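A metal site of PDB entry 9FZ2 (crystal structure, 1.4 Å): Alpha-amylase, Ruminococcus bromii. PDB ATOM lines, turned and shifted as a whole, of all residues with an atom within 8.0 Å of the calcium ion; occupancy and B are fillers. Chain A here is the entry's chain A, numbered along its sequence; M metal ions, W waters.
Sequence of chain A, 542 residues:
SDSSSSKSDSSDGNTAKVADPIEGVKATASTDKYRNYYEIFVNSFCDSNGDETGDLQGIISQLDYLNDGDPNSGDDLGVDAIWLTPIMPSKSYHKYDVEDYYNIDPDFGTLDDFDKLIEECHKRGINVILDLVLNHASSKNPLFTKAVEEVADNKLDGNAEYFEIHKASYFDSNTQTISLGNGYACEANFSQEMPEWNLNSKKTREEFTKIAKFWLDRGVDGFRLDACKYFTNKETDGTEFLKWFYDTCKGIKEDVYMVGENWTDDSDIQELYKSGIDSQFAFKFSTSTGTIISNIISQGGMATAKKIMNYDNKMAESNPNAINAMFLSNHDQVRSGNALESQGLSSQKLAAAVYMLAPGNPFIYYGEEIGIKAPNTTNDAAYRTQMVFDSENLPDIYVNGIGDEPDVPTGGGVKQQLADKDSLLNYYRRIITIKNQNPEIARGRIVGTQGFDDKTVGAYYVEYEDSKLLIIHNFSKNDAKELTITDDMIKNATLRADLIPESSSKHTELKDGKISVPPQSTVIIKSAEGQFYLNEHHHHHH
The calcium ion is bound by O of Ser 73 (2.2 Å), O of Asp 70 (2.3 Å), OD1 of Asp 76 (2.3 Å), water W1 (2.4 Å), OD1 of Asp 68 (2.5 Å) and OD2 of Asp 68 (2.9 Å). Slightly farther from the calcium ion lies water W2 (2.9 Å).
OD2 of Asp 70 lies within hydrogen-bond range of OG of Ser 73 (2.7 Å). The backbone NH of Asn 72 lies within hydrogen-bond range of the side-chain carboxylate of Asp 70. NE of Arg 429 sits at hydrogen-bond distance from O of Asp 76.
Four residues have an atom within 4 Å of the calcium ion: Asp 68, Asp 70, Ser 73 and Asp 76. The nearest printed residue that does not touch the calcium ion is Gly 74 (4.2 Å).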
ATOM      1  N   ASP A  64     -32.039  31.432  16.189  1.00  0.00           N
ATOM      2  CA  ASP A  64     -31.560  30.138  16.662  1.00  0.00           C
ATOM      3  C   ASP A  64     -30.035  30.056  16.740  1.00  0.00           C
ATOM      4  O   ASP A  64     -29.510  29.226  17.487  1.00  0.00           O
ATOM      5  CB  ASP A  64     -32.062  28.982  15.821  1.00  0.00           C
ATOM      6  CG  ASP A  64     -33.375  28.370  16.277  1.00  0.00           C
ATOM      7  OD1 ASP A  64     -33.986  28.863  17.257  1.00  0.00           O
ATOM      8  OD2 ASP A  64     -33.725  27.331  15.671  1.00  0.00           O
ATOM      9  N   TYR A  65     -29.319  30.862  15.928  1.00  0.00           N
ATOM     10  CA  TYR A  65     -27.878  31.016  16.112  1.00  0.00           C
ATOM     11  C   TYR A  65     -27.571  31.677  17.462  1.00  0.00           C
ATOM     12  O   TYR A  65     -26.741  31.204  18.226  1.00  0.00           O
ATOM     13  CB  TYR A  65     -27.238  31.837  14.994  1.00  0.00           C
ATOM     14  CG  TYR A  65     -25.849  32.357  15.334  1.00  0.00           C
ATOM     15  CD1 TYR A  65     -24.816  31.476  15.661  1.00  0.00           C
ATOM     16  CD2 TYR A  65     -25.574  33.719  15.439  1.00  0.00           C
ATOM     17  CE1 TYR A  65     -23.563  31.929  16.011  1.00  0.00           C
ATOM     18  CE2 TYR A  65     -24.319  34.181  15.785  1.00  0.00           C
ATOM     19  CZ  TYR A  65     -23.304  33.280  16.076  1.00  0.00           C
ATOM     20  OH  TYR A  65     -22.048  33.670  16.402  1.00  0.00           O
ATOM     21  N   LEU A  66     -28.291  32.729  17.826  1.00  0.00           N
ATOM     22  CA  LEU A  66     -28.067  33.375  19.089  1.00  0.00           C
ATOM     23  C   LEU A  66     -28.422  32.497  20.291  1.00  0.00           C
ATOM     24  O   LEU A  66     -27.628  32.396  21.208  1.00  0.00           O
ATOM     25  CB  LEU A  66     -28.820  34.701  19.079  1.00  0.00           C
ATOM     26  CG  LEU A  66     -28.283  35.701  18.048  1.00  0.00           C
ATOM     27  CD1 LEU A  66     -28.972  37.061  18.172  1.00  0.00           C
ATOM     28  CD2 LEU A  66     -26.771  35.852  18.169  1.00  0.00           C
ATOM     29  N   ASN A  67     -29.597  31.853  20.300  1.00  0.00           N
ATOM     30  CA  ASN A  67     -29.958  30.984  21.402  1.00  0.00           C
ATOM     31  C   ASN A  67     -31.071  30.064  20.902  1.00  0.00           C
ATOM     32  O   ASN A  67     -32.061  30.568  20.385  1.00  0.00           O
ATOM     33  CB  ASN A  67     -30.486  31.761  22.594  1.00  0.00           C
ATOM     34  CG  ASN A  67     -30.465  30.973  23.891  1.00  0.00           C
ATOM     35  OD1 ASN A  67     -30.863  29.796  23.940  1.00  0.00           O
ATOM     36  ND2 ASN A  67     -29.965  31.590  24.944  1.00  0.00           N
ATOM     37  N   ASP A  68     -30.867  28.759  20.978  1.00  0.00           N
ATOM     38  CA  ASP A  68     -31.878  27.808  20.505  1.00  0.00           C
ATOM     39  C   ASP A  68     -32.858  27.429  21.623  1.00  0.00           C
ATOM     40  O   ASP A  68     -33.750  26.604  21.421  1.00  0.00           O
ATOM     41  CB  ASP A  68     -31.232  26.595  19.855  1.00  0.00           C
ATOM     42  CG  ASP A  68     -30.405  25.763  20.823  1.00  0.00           C
ATOM     43  OD1 ASP A  68     -30.471  26.056  22.022  1.00  0.00           O
ATOM     44  OD2 ASP A  68     -29.723  24.816  20.366  1.00  0.00           O
ATOM     45  N   GLY A  69     -32.651  27.943  22.835  1.00  0.00           N
ATOM     46  CA  GLY A  69     -33.599  27.731  23.925  1.00  0.00           C
ATOM     47  C   GLY A  69     -33.314  26.476  24.741  1.00  0.00           C
ATOM     48  O   GLY A  69     -34.040  26.182  25.687  1.00  0.00           O
ATOM     49  N   ASP A  70     -32.296  25.704  24.353  1.00  0.00           N
ATOM     50  CA  ASP A  70     -31.904  24.518  25.087  1.00  0.00           C
ATOM     51  C   ASP A  70     -30.429  24.589  25.453  1.00  0.00           C
ATOM     52  O   ASP A  70     -29.565  24.287  24.632  1.00  0.00           O
ATOM     53  CB  ASP A  70     -32.129  23.236  24.285  1.00  0.00           C
ATOM     54  CG  ASP A  70     -31.766  21.938  25.022  1.00  0.00           C
ATOM     55  OD1 ASP A  70     -31.259  21.992  26.160  1.00  0.00           O
ATOM     56  OD2 ASP A  70     -32.005  20.878  24.446  1.00  0.00           O
ATOM     57  N   PRO A  71     -30.113  24.959  26.714  1.00  0.00           N
ATOM     58  CA  PRO A  71     -28.716  25.074  27.130  1.00  0.00           C
ATOM     59  C   PRO A  71     -27.914  23.777  27.157  1.00  0.00           C
ATOM     60  O   PRO A  71     -26.702  23.828  27.383  1.00  0.00           O
ATOM     61  CB  PRO A  71     -28.828  25.729  28.539  1.00  0.00           C
ATOM     62  CG  PRO A  71     -30.183  25.350  29.054  1.00  0.00           C
ATOM     63  CD  PRO A  71     -31.064  25.297  27.805  1.00  0.00           C
ATOM     64  N   ASN A  72     -28.560  22.624  26.923  1.00  0.00           N
ATOM     65  CA  ASN A  72     -27.900  21.335  27.047  1.00  0.00           C
ATOM     66  C   ASN A  72     -27.686  20.648  25.694  1.00  0.00           C
ATOM     67  O   ASN A  72     -27.191  19.514  25.679  1.00  0.00           O
ATOM     68  CB  ASN A  72     -28.658  20.459  28.035  1.00  0.00           C
ATOM     69  CG  ASN A  72     -28.446  20.967  29.449  1.00  0.00           C
ATOM     70  OD1 ASN A  72     -27.307  20.939  29.931  1.00  0.00           O
ATOM     71  ND2 ASN A  72     -29.474  21.461  30.112  1.00  0.00           N
ATOM     72  N   SER A  73     -28.037  21.296  24.586  1.00  0.00           N
ATOM     73  CA  SER A  73     -27.771  20.693  23.285  1.00  0.00           C
ATOM     74  C   SER A  73     -27.702  21.802  22.247  1.00  0.00           C
ATOM     75  O   SER A  73     -28.055  22.926  22.556  1.00  0.00           O
ATOM     76  CB  SER A  73     -28.812  19.695  22.941  1.00  0.00           C
ATOM     77  OG  SER A  73     -30.038  20.360  22.661  1.00  0.00           O
ATOM     78  N   GLY A  74     -27.217  21.475  21.056  1.00  0.00           N
ATOM     79  CA  GLY A  74     -27.258  22.350  19.903  1.00  0.00           C
ATOM     80  C   GLY A  74     -25.896  22.994  19.627  1.00  0.00           C
ATOM     81  O   GLY A  74     -24.901  22.589  20.216  1.00  0.00           O
ATOM     82  N   ASP A  75     -25.846  23.929  18.665  1.00  0.00           N
ATOM     83  CA  ASP A  75     -24.606  24.616  18.323  1.00  0.00           C
ATOM     84  C   ASP A  75     -24.873  26.115  18.156  1.00  0.00           C
ATOM     85  O   ASP A  75     -24.309  26.802  17.289  1.00  0.00           O
ATOM     86  CB  ASP A  75     -23.943  24.055  17.086  1.00  0.00           C
ATOM     87  CG  ASP A  75     -24.774  24.149  15.822  1.00  0.00           C
ATOM     88  OD1 ASP A  75     -25.935  24.553  15.940  1.00  0.00           O
ATOM     89  OD2 ASP A  75     -24.252  23.795  14.727  1.00  0.00           O
ATOM     90  N   ASP A  76     -25.710  26.628  19.039  1.00  0.00           N
ATOM     91  CA  ASP A  76     -25.972  28.041  19.117  1.00  0.00           C
ATOM     92  C   ASP A  76     -24.876  28.690  19.941  1.00  0.00           C
ATOM     93  O   ASP A  76     -24.229  28.043  20.753  1.00  0.00           O
ATOM     94  CB  ASP A  76     -27.343  28.214  19.753  1.00  0.00           C
ATOM     95  CG  ASP A  76     -27.495  27.610  21.141  1.00  0.00           C
ATOM     96  OD1 ASP A  76     -27.098  26.415  21.361  1.00  0.00           O
ATOM     97  OD2 ASP A  76     -28.086  28.318  22.009  1.00  0.00           O
ATOM     98  N   LEU A  77     -24.704  30.000  19.749  1.00  0.00           N
ATOM     99  CA  LEU A  77     -23.800  30.809  20.554  1.00  0.00           C
ATOM    100  C   LEU A  77     -24.199  30.680  22.029  1.00  0.00           C
ATOM    101  O   LEU A  77     -23.356  30.456  22.865  1.00  0.00           O
ATOM    102  CB  LEU A  77     -23.831  32.261  20.073  1.00  0.00           C
ATOM    103  CG  LEU A  77     -23.001  33.285  20.870  1.00  0.00           C
ATOM    104  CD1 LEU A  77     -21.549  32.860  20.972  1.00  0.00           C
ATOM    105  CD2 LEU A  77     -23.156  34.651  20.195  1.00  0.00           C
ATOM    106  N   GLY A  78     -25.450  30.989  22.350  1.00  0.00           N
ATOM    107  CA  GLY A  78     -25.952  30.812  23.691  1.00  0.00           C
ATOM    108  C   GLY A  78     -26.252  32.102  24.411  1.00  0.00           C
ATOM    109  O   GLY A  78     -26.596  32.037  25.577  1.00  0.00           O
ATOM    110  N   ARG A 429     -18.762  29.785  23.004  1.00  0.00           N
ATOM    111  CA  ARG A 429     -19.870  28.890  23.288  1.00  0.00           C
ATOM    112  C   ARG A 429     -19.580  28.147  24.582  1.00  0.00           C
ATOM    113  O   ARG A 429     -20.485  27.974  25.409  1.00  0.00           O
ATOM    114  CB  ARG A 429     -20.122  27.873  22.182  1.00  0.00           C
ATOM    115  CG  ARG A 429     -20.810  28.527  20.997  1.00  0.00           C
ATOM    116  CD  ARG A 429     -21.078  27.545  19.858  1.00  0.00           C
ATOM    117  NE  ARG A 429     -21.921  26.454  20.370  1.00  0.00           N
ATOM    118  CZ  ARG A 429     -21.549  25.237  20.757  1.00  0.00           C
ATOM    119  NH1 ARG A 429     -20.352  24.762  20.459  1.00  0.00           N
ATOM    120  NH2 ARG A 429     -22.381  24.466  21.453  1.00  0.00           N
ATOM    121  N   THR A 433     -21.546  28.035  28.292  1.00  0.00           N
ATOM    122  CA  THR A 433     -21.979  26.790  28.927  1.00  0.00           C
ATOM    123  C   THR A 433     -21.438  26.683  30.364  1.00  0.00           C
ATOM    124  O   THR A 433     -22.200  26.430  31.283  1.00  0.00           O
ATOM    125  CB  THR A 433     -21.563  25.621  28.031  1.00  0.00           C
ATOM    126  OG1 THR A 433     -22.343  25.721  26.844  1.00  0.00           O
ATOM    127  CG2 THR A 433     -21.837  24.302  28.726  1.00  0.00           C
ATOM    128  N   ASN A 436     -23.490  28.865  32.489  1.00  0.00           N
ATOM    129  CA  ASN A 436     -24.804  28.246  32.708  1.00  0.00           C
ATOM    130  C   ASN A 436     -24.726  27.035  33.658  1.00  0.00           C
ATOM    131  O   ASN A 436     -25.761  26.484  34.038  1.00  0.00           O
ATOM    132  CB  ASN A 436     -25.426  27.777  31.396  1.00  0.00           C
ATOM    133  CG  ASN A 436     -25.877  28.880  30.455  1.00  0.00           C
ATOM    134  OD1 ASN A 436     -26.121  30.008  30.867  1.00  0.00           O
ATOM    135  ND2 ASN A 436     -26.027  28.550  29.185  1.00  0.00           N
HETATM  136 CA    CA M   1     -28.348  25.113  22.861  1.00  0.00          CA
HETATM  137  O   HOH W   1     -27.892  27.044  24.259  1.00  0.00           O
HETATM  138  O   HOH W   2     -25.803  24.682  24.255  1.00  0.00           O
